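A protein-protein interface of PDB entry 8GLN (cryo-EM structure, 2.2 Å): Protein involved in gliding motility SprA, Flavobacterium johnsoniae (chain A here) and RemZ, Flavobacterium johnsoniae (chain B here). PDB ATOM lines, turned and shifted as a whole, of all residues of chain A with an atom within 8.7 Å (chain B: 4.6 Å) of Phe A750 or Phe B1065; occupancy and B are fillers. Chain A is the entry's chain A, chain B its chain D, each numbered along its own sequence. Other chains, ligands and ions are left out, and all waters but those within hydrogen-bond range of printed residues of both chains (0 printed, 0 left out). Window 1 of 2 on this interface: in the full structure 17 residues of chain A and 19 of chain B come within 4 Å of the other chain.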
ATOM      1  N   PHE A 199     -21.399  17.622 -25.351  1.00  0.00           N
ATOM      2  CA  PHE A 199     -20.325  17.337 -26.297  1.00  0.00           C
ATOM      3  C   PHE A 199     -20.089  15.844 -26.498  1.00  0.00           C
ATOM      4  O   PHE A 199     -20.370  15.314 -27.578  1.00  0.00           O
ATOM      5  CB  PHE A 199     -19.023  17.991 -25.823  1.00  0.00           C
ATOM      6  CG  PHE A 199     -19.061  19.493 -25.810  1.00  0.00           C
ATOM      7  CD1 PHE A 199     -20.024  20.188 -26.522  1.00  0.00           C
ATOM      8  CD2 PHE A 199     -18.127  20.211 -25.080  1.00  0.00           C
ATOM      9  CE1 PHE A 199     -20.056  21.569 -26.506  1.00  0.00           C
ATOM     10  CE2 PHE A 199     -18.154  21.591 -25.061  1.00  0.00           C
ATOM     11  CZ  PHE A 199     -19.120  22.271 -25.775  1.00  0.00           C
ATOM     12  N   ALA A 200     -19.584  15.150 -25.478  1.00  0.00           N
ATOM     13  CA  ALA A 200     -19.364  13.712 -25.615  1.00  0.00           C
ATOM     14  C   ALA A 200     -19.700  12.879 -24.387  1.00  0.00           C
ATOM     15  O   ALA A 200     -19.834  11.658 -24.528  1.00  0.00           O
ATOM     16  CB  ALA A 200     -17.907  13.434 -26.008  1.00  0.00           C
ATOM     17  N   LYS A 262     -11.518  11.741 -20.824  1.00  0.00           N
ATOM     18  CA  LYS A 262     -12.389  12.716 -21.463  1.00  0.00           C
ATOM     19  C   LYS A 262     -12.443  14.044 -20.721  1.00  0.00           C
ATOM     20  O   LYS A 262     -13.072  14.985 -21.213  1.00  0.00           O
ATOM     21  CB  LYS A 262     -13.807  12.150 -21.593  1.00  0.00           C
ATOM     22  CG  LYS A 262     -13.862  10.752 -22.175  1.00  0.00           C
ATOM     23  CD  LYS A 262     -13.188  10.693 -23.530  1.00  0.00           C
ATOM     24  CE  LYS A 262     -13.215   9.285 -24.092  1.00  0.00           C
ATOM     25  NZ  LYS A 262     -14.058   9.187 -25.313  1.00  0.00           N
ATOM     26  N   GLN A 264     -10.494  17.232 -18.145  1.00  0.00           N
ATOM     27  CA  GLN A 264      -9.285  18.013 -17.947  1.00  0.00           C
ATOM     28  C   GLN A 264      -9.270  18.541 -16.522  1.00  0.00           C
ATOM     29  O   GLN A 264     -10.284  19.040 -16.027  1.00  0.00           O
ATOM     30  CB  GLN A 264      -9.207  19.175 -18.944  1.00  0.00           C
ATOM     31  CG  GLN A 264      -7.991  20.062 -18.778  1.00  0.00           C
ATOM     32  CD  GLN A 264      -7.790  20.991 -19.957  1.00  0.00           C
ATOM     33  OE1 GLN A 264      -8.262  22.128 -19.954  1.00  0.00           O
ATOM     34  NE2 GLN A 264      -7.087  20.511 -20.977  1.00  0.00           N
ATOM     35  N   ASN A 746     -12.745  18.725 -15.317  1.00  0.00           N
ATOM     36  CA  ASN A 746     -13.595  19.477 -16.233  1.00  0.00           C
ATOM     37  C   ASN A 746     -13.798  18.634 -17.485  1.00  0.00           C
ATOM     38  O   ASN A 746     -12.852  18.410 -18.248  1.00  0.00           O
ATOM     39  CB  ASN A 746     -12.969  20.829 -16.570  1.00  0.00           C
ATOM     40  CG  ASN A 746     -13.922  21.748 -17.310  1.00  0.00           C
ATOM     41  OD1 ASN A 746     -15.015  21.345 -17.704  1.00  0.00           O
ATOM     42  ND2 ASN A 746     -13.507  22.993 -17.504  1.00  0.00           N
ATOM     43  N   ASN A 747     -15.026  18.165 -17.692  1.00  0.00           N
ATOM     44  CA  ASN A 747     -15.375  17.408 -18.886  1.00  0.00           C
ATOM     45  C   ASN A 747     -16.111  18.252 -19.919  1.00  0.00           C
ATOM     46  O   ASN A 747     -16.572  17.714 -20.929  1.00  0.00           O
ATOM     47  CB  ASN A 747     -16.198  16.171 -18.511  1.00  0.00           C
ATOM     48  CG  ASN A 747     -17.458  16.509 -17.734  1.00  0.00           C
ATOM     49  OD1 ASN A 747     -18.083  17.549 -17.945  1.00  0.00           O
ATOM     50  ND2 ASN A 747     -17.842  15.618 -16.828  1.00  0.00           N
ATOM     51  N   SER A 748     -16.233  19.554 -19.687  1.00  0.00           N
ATOM     52  CA  SER A 748     -16.812  20.474 -20.665  1.00  0.00           C
ATOM     53  C   SER A 748     -15.707  21.127 -21.493  1.00  0.00           C
ATOM     54  O   SER A 748     -15.553  22.347 -21.537  1.00  0.00           O
ATOM     55  CB  SER A 748     -17.672  21.521 -19.962  1.00  0.00           C
ATOM     56  OG  SER A 748     -18.587  20.915 -19.066  1.00  0.00           O
ATOM     57  N   ILE A 749     -14.927  20.281 -22.159  1.00  0.00           N
ATOM     58  CA  ILE A 749     -13.774  20.718 -22.932  1.00  0.00           C
ATOM     59  C   ILE A 749     -13.968  20.309 -24.383  1.00  0.00           C
ATOM     60  O   ILE A 749     -14.697  19.360 -24.692  1.00  0.00           O
ATOM     61  CB  ILE A 749     -12.455  20.141 -22.372  1.00  0.00           C
ATOM     62  CG1 ILE A 749     -12.438  18.617 -22.516  1.00  0.00           C
ATOM     63  CG2 ILE A 749     -12.268  20.550 -20.920  1.00  0.00           C
ATOM     64  CD1 ILE A 749     -11.280  17.945 -21.817  1.00  0.00           C
ATOM     65  N   PHE A 750     -13.308  21.038 -25.278  1.00  0.00           N
ATOM     66  CA  PHE A 750     -13.416  20.784 -26.706  1.00  0.00           C
ATOM     67  C   PHE A 750     -12.106  21.166 -27.378  1.00  0.00           C
ATOM     68  O   PHE A 750     -11.323  21.959 -26.850  1.00  0.00           O
ATOM     69  CB  PHE A 750     -14.589  21.558 -27.324  1.00  0.00           C
ATOM     70  CG  PHE A 750     -14.568  23.030 -27.025  1.00  0.00           C
ATOM     71  CD1 PHE A 750     -13.830  23.901 -27.809  1.00  0.00           C
ATOM     72  CD2 PHE A 750     -15.282  23.543 -25.956  1.00  0.00           C
ATOM     73  CE1 PHE A 750     -13.807  25.253 -27.534  1.00  0.00           C
ATOM     74  CE2 PHE A 750     -15.263  24.895 -25.679  1.00  0.00           C
ATOM     75  CZ  PHE A 750     -14.526  25.750 -26.468  1.00  0.00           C
ATOM     76  N   GLY A 751     -11.880  20.593 -28.557  1.00  0.00           N
ATOM     77  CA  GLY A 751     -10.677  20.893 -29.313  1.00  0.00           C
ATOM     78  C   GLY A 751      -9.395  20.495 -28.621  1.00  0.00           C
ATOM     79  O   GLY A 751      -8.354  21.119 -28.851  1.00  0.00           O
ATOM     80  N   GLN A 752      -9.438  19.469 -27.780  1.00  0.00           N
ATOM     81  CA  GLN A 752      -8.276  19.021 -27.029  1.00  0.00           C
ATOM     82  C   GLN A 752      -7.689  17.758 -27.647  1.00  0.00           C
ATOM     83  O   GLN A 752      -8.349  17.035 -28.395  1.00  0.00           O
ATOM     84  CB  GLN A 752      -8.641  18.766 -25.564  1.00  0.00           C
ATOM     85  CG  GLN A 752      -9.520  19.838 -24.930  1.00  0.00           C
ATOM     86  CD  GLN A 752      -8.754  21.091 -24.546  1.00  0.00           C
ATOM     87  OE1 GLN A 752      -7.971  21.627 -25.331  1.00  0.00           O
ATOM     88  NE2 GLN A 752      -8.981  21.567 -23.328  1.00  0.00           N
ATOM     89  N   GLN A 753      -6.426  17.504 -27.320  1.00  0.00           N
ATOM     90  CA  GLN A 753      -5.756  16.304 -27.791  1.00  0.00           C
ATOM     91  C   GLN A 753      -6.332  15.066 -27.112  1.00  0.00           C
ATOM     92  O   GLN A 753      -6.870  15.131 -26.004  1.00  0.00           O
ATOM     93  CB  GLN A 753      -4.255  16.388 -27.524  1.00  0.00           C
ATOM     94  CG  GLN A 753      -3.616  17.696 -27.947  1.00  0.00           C
ATOM     95  CD  GLN A 753      -2.189  17.822 -27.457  1.00  0.00           C
ATOM     96  OE1 GLN A 753      -1.414  16.870 -27.520  1.00  0.00           O
ATOM     97  NE2 GLN A 753      -1.835  19.000 -26.959  1.00  0.00           N
ATOM     98  N   PHE A 784      -2.009  16.637 -32.317  1.00  0.00           N
ATOM     99  CA  PHE A 784      -2.744  16.714 -33.577  1.00  0.00           C
ATOM    100  C   PHE A 784      -1.814  16.486 -34.762  1.00  0.00           C
ATOM    101  O   PHE A 784      -2.140  15.737 -35.689  1.00  0.00           O
ATOM    102  CB  PHE A 784      -3.442  18.069 -33.690  1.00  0.00           C
ATOM    103  CG  PHE A 784      -4.528  18.279 -32.674  1.00  0.00           C
ATOM    104  CD1 PHE A 784      -5.413  17.261 -32.364  1.00  0.00           C
ATOM    105  CD2 PHE A 784      -4.664  19.497 -32.029  1.00  0.00           C
ATOM    106  CE1 PHE A 784      -6.413  17.453 -31.430  1.00  0.00           C
ATOM    107  CE2 PHE A 784      -5.662  19.696 -31.095  1.00  0.00           C
ATOM    108  CZ  PHE A 784      -6.537  18.672 -30.794  1.00  0.00           C
ATOM    109  N   SER B1063     -13.570  30.495 -30.085  1.00  0.00           N
ATOM    110  CA  SER B1063     -12.702  29.619 -30.859  1.00  0.00           C
ATOM    111  C   SER B1063     -13.443  29.209 -32.120  1.00  0.00           C
ATOM    112  O   SER B1063     -14.555  28.677 -32.043  1.00  0.00           O
ATOM    113  CB  SER B1063     -12.288  28.390 -30.046  1.00  0.00           C
ATOM    114  OG  SER B1063     -11.666  28.770 -28.833  1.00  0.00           O
ATOM    115  N   ILE B1064     -12.831  29.454 -33.274  1.00  0.00           N
ATOM    116  CA  ILE B1064     -13.430  29.138 -34.564  1.00  0.00           C
ATOM    117  C   ILE B1064     -12.714  27.929 -35.143  1.00  0.00           C
ATOM    118  O   ILE B1064     -11.483  27.921 -35.257  1.00  0.00           O
ATOM    119  CB  ILE B1064     -13.355  30.339 -35.523  1.00  0.00           C
ATOM    120  CG1 ILE B1064     -14.163  31.513 -34.965  1.00  0.00           C
ATOM    121  CG2 ILE B1064     -13.857  29.955 -36.903  1.00  0.00           C
ATOM    122  CD1 ILE B1064     -13.801  32.842 -35.574  1.00  0.00           C
ATOM    123  N   PHE B1065     -13.481  26.906 -35.501  1.00  0.00           N
ATOM    124  CA  PHE B1065     -12.937  25.654 -36.003  1.00  0.00           C
ATOM    125  C   PHE B1065     -13.412  25.402 -37.426  1.00  0.00           C
ATOM    126  O   PHE B1065     -14.596  25.563 -37.735  1.00  0.00           O
ATOM    127  CB  PHE B1065     -13.350  24.471 -35.120  1.00  0.00           C
ATOM    128  CG  PHE B1065     -12.828  24.543 -33.716  1.00  0.00           C
ATOM    129  CD1 PHE B1065     -13.503  25.265 -32.747  1.00  0.00           C
ATOM    130  CD2 PHE B1065     -11.666  23.881 -33.361  1.00  0.00           C
ATOM    131  CE1 PHE B1065     -13.027  25.329 -31.454  1.00  0.00           C
ATOM    132  CE2 PHE B1065     -11.185  23.940 -32.069  1.00  0.00           C
ATOM    133  CZ  PHE B1065     -11.866  24.667 -31.115  1.00  0.00           C
ATOM    134  N   ASP B1066     -12.478  25.010 -38.287  1.00  0.00           N
ATOM    135  CA  ASP B1066     -12.837  24.384 -39.547  1.00  0.00           C
ATOM    136  C   ASP B1066     -13.425  23.014 -39.221  1.00  0.00           C
ATOM    137  O   ASP B1066     -13.199  22.461 -38.142  1.00  0.00           O
ATOM    138  CB  ASP B1066     -11.588  24.317 -40.449  1.00  0.00           C
ATOM    139  CG  ASP B1066     -11.657  23.263 -41.568  1.00  0.00           C
ATOM    140  OD1 ASP B1066     -12.645  22.519 -41.724  1.00  0.00           O
ATOM    141  OD2 ASP B1066     -10.667  23.185 -42.327  1.00  0.00           O
ATOM    142  N   ILE B1067     -14.190  22.453 -40.156  1.00  0.00           N
ATOM    143  CA  ILE B1067     -14.792  21.163 -39.847  1.00  0.00           C
ATOM    144  C   ILE B1067     -13.769  20.083 -40.162  1.00  0.00           C
ATOM    145  O   ILE B1067     -13.911  19.313 -41.118  1.00  0.00           O
ATOM    146  CB  ILE B1067     -16.095  20.959 -40.641  1.00  0.00           C
ATOM    147  CG1 ILE B1067     -15.913  21.457 -42.077  1.00  0.00           C
ATOM    148  CG2 ILE B1067     -17.248  21.676 -39.963  1.00  0.00           C
ATOM    149  CD1 ILE B1067     -17.069  21.156 -42.988  1.00  0.00           C
ATOM    150  N   GLY B1069     -11.775  19.471 -36.866  1.00  0.00           N
ATOM    151  CA  GLY B1069     -11.127  19.583 -35.581  1.00  0.00           C
ATOM    152  C   GLY B1069     -10.013  20.604 -35.529  1.00  0.00           C
ATOM    153  O   GLY B1069      -9.438  20.813 -34.453  1.00  0.00           O
ATOM    154  N   LYS B1070      -9.693  21.250 -36.649  1.00  0.00           N
ATOM    155  CA  LYS B1070      -8.580  22.188 -36.704  1.00  0.00           C
ATOM    156  C   LYS B1070      -9.019  23.570 -36.234  1.00  0.00           C
ATOM    157  O   LYS B1070     -10.007  24.121 -36.728  1.00  0.00           O
ATOM    158  CB  LYS B1070      -8.023  22.270 -38.124  1.00  0.00           C
ATOM    159  CG  LYS B1070      -6.913  23.293 -38.294  1.00  0.00           C
ATOM    160  CD  LYS B1070      -6.324  23.244 -39.693  1.00  0.00           C
ATOM    161  CE  LYS B1070      -5.524  24.497 -40.002  1.00  0.00           C
ATOM    162  NZ  LYS B1070      -4.856  25.040 -38.786  1.00  0.00           N
ATOM    163  N   LEU B1071      -8.273  24.129 -35.287  1.00  0.00           N
ATOM    164  CA  LEU B1071      -8.547  25.466 -34.777  1.00  0.00           C
ATOM    165  C   LEU B1071      -7.942  26.506 -35.710  1.00  0.00           C
ATOM    166  O   LEU B1071      -6.724  26.525 -35.921  1.00  0.00           O
ATOM    167  CB  LEU B1071      -7.988  25.618 -33.364  1.00  0.00           C
ATOM    168  CG  LEU B1071      -8.129  26.995 -32.718  1.00  0.00           C
ATOM    169  CD1 LEU B1071      -9.526  27.185 -32.154  1.00  0.00           C
ATOM    170  CD2 LEU B1071      -7.081  27.183 -31.634  1.00  0.00           C
ATOM    171  N   LEU B1072      -8.788  27.372 -36.268  1.00  0.00           N
ATOM    172  CA  LEU B1072      -8.330  28.435 -37.151  1.00  0.00           C
ATOM    173  C   LEU B1072      -8.165  29.774 -36.450  1.00  0.00           C
ATOM    174  O   LEU B1072      -7.388  30.610 -36.922  1.00  0.00           O
ATOM    175  CB  LEU B1072      -9.302  28.618 -38.321  1.00  0.00           C
ATOM    176  CG  LEU B1072      -9.710  27.376 -39.108  1.00  0.00           C
ATOM    177  CD1 LEU B1072     -10.698  27.764 -40.189  1.00  0.00           C
ATOM    178  CD2 LEU B1072      -8.490  26.704 -39.707  1.00  0.00           C
ATOM    179  N   LEU B1095     -17.834  26.610 -40.977  1.00  0.00           N
ATOM    180  CA  LEU B1095     -17.044  26.839 -39.778  1.00  0.00           C
ATOM    181  C   LEU B1095     -17.907  26.609 -38.548  1.00  0.00           C
ATOM    182  O   LEU B1095     -19.130  26.763 -38.591  1.00  0.00           O
ATOM    183  CB  LEU B1095     -16.473  28.262 -39.741  1.00  0.00           C
ATOM    184  CG  LEU B1095     -15.401  28.603 -40.771  1.00  0.00           C
ATOM    185  CD1 LEU B1095     -14.814  29.969 -40.486  1.00  0.00           C
ATOM    186  CD2 LEU B1095     -14.319  27.547 -40.738  1.00  0.00           C
ATOM    187  N   ILE B1096     -17.259  26.241 -37.448  1.00  0.00           N
ATOM    188  CA  ILE B1096     -17.921  26.051 -36.163  1.00  0.00           C
ATOM    189  C   ILE B1096     -17.394  27.107 -35.205  1.00  0.00           C
ATOM    190  O   ILE B1096     -16.187  27.169 -34.941  1.00  0.00           O
ATOM    191  CB  ILE B1096     -17.692  24.640 -35.604  1.00  0.00           C
ATOM    192  CG1 ILE B1096     -18.237  23.588 -36.569  1.00  0.00           C
ATOM    193  CG2 ILE B1096     -18.347  24.500 -34.241  1.00  0.00           C
ATOM    194  CD1 ILE B1096     -17.864  22.178 -36.195  1.00  0.00           C
ATOM    195  N   LYS B1098     -17.404  28.410 -31.429  1.00  0.00           N
ATOM    196  CA  LYS B1098     -17.664  28.047 -30.043  1.00  0.00           C
ATOM    197  C   LYS B1098     -17.301  29.233 -29.165  1.00  0.00           C
ATOM    198  O   LYS B1098     -16.161  29.707 -29.197  1.00  0.00           O
ATOM    199  CB  LYS B1098     -16.876  26.802 -29.637  1.00  0.00           C
ATOM    200  CG  LYS B1098     -17.273  25.556 -30.406  1.00  0.00           C
ATOM    201  CD  LYS B1098     -16.785  24.301 -29.715  1.00  0.00           C
ATOM    202  CE  LYS B1098     -17.665  23.955 -28.531  1.00  0.00           C
ATOM    203  NZ  LYS B1098     -19.020  23.517 -28.952  1.00  0.00           N
ATOM    204  N   THR B1100     -17.265  30.844 -25.299  1.00  0.00           N
ATOM    205  CA  THR B1100     -17.326  30.637 -23.859  1.00  0.00           C
ATOM    206  C   THR B1100     -17.839  31.913 -23.205  1.00  0.00           C
ATOM    207  O   THR B1100     -17.217  32.973 -23.327  1.00  0.00           O
ATOM    208  CB  THR B1100     -15.956  30.261 -23.301  1.00  0.00           C
ATOM    209  OG1 THR B1100     -15.481  29.076 -23.951  1.00  0.00           O
ATOM    210  CG2 THR B1100     -16.044  30.012 -21.804  1.00  0.00           C
ATOM    211  N   ILE B1106     -21.135  27.342 -22.785  1.00  0.00           N
ATOM    212  CA  ILE B1106     -20.493  27.280 -24.093  1.00  0.00           C
ATOM    213  C   ILE B1106     -21.587  27.236 -25.149  1.00  0.00           C
ATOM    214  O   ILE B1106     -22.447  26.348 -25.128  1.00  0.00           O
ATOM    215  CB  ILE B1106     -19.560  26.067 -24.206  1.00  0.00           C
ATOM    216  CG1 ILE B1106     -18.603  26.026 -23.014  1.00  0.00           C
ATOM    217  CG2 ILE B1106     -18.786  26.111 -25.512  1.00  0.00           C
ATOM    218  CD1 ILE B1106     -17.631  24.874 -23.049  1.00  0.00           C
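The backbone NH (N) of Ser A748 is in hydrogen-bond range of the side-chain amide oxygen (OD1) of Asn A746 (2.9 Å).
The backbone NH of Ser B1063 is in hydrogen-bond range of the backbone carbonyl oxygen of Lys B1098.
The backbone carbonyl oxygen (O) of Phe B1065 is in hydrogen-bond range of the backbone NH (N) of Ile B1096, 2.8 Å away.
Of the 13 printed residues of chain A, 3 touch a printed residue of chain B.
Printed residues of chain A that touch a printed residue of chain B: Phe A199, Ser A748 and Phe A750.
Hydrophobic or aromatic side chains of chain A within 4 Å of the printed part of chain B: Phe A199 and Phe A750.
Among the printed residues, 6 pairs touch across the chains.
Lys B1098 touches Phe A199.
CZ of Phe A199 touches CG2 of Ile B1106 (3.9 Å).
O of Ser A748 touches CD1 of Ile B1106, 3.6 Å away.
CZ of Phe B1065 touches CD1 of Phe A750 (3.9 Å).
Phe A750 touches Lys B1098.
Ile B1106 touches Phe A750 (CD1 to CE2, 3.5 Å).
Printed residues of chain B within 4 Å of Ser A748: Ile B1106 (3.6 Å).
Phe A750 touches just these residues of chain B: Phe B1065, Lys B1098 and Ile B1106.
Phe B1065 touches just one residue of chain A: Phe A750.
Printed residues of chain A within 4 Å of Lys B1098: Phe A199 and Phe A750.
The nearest residue of chain A that does not touch Phe B1065 is Gly A751 (4.1 Å).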
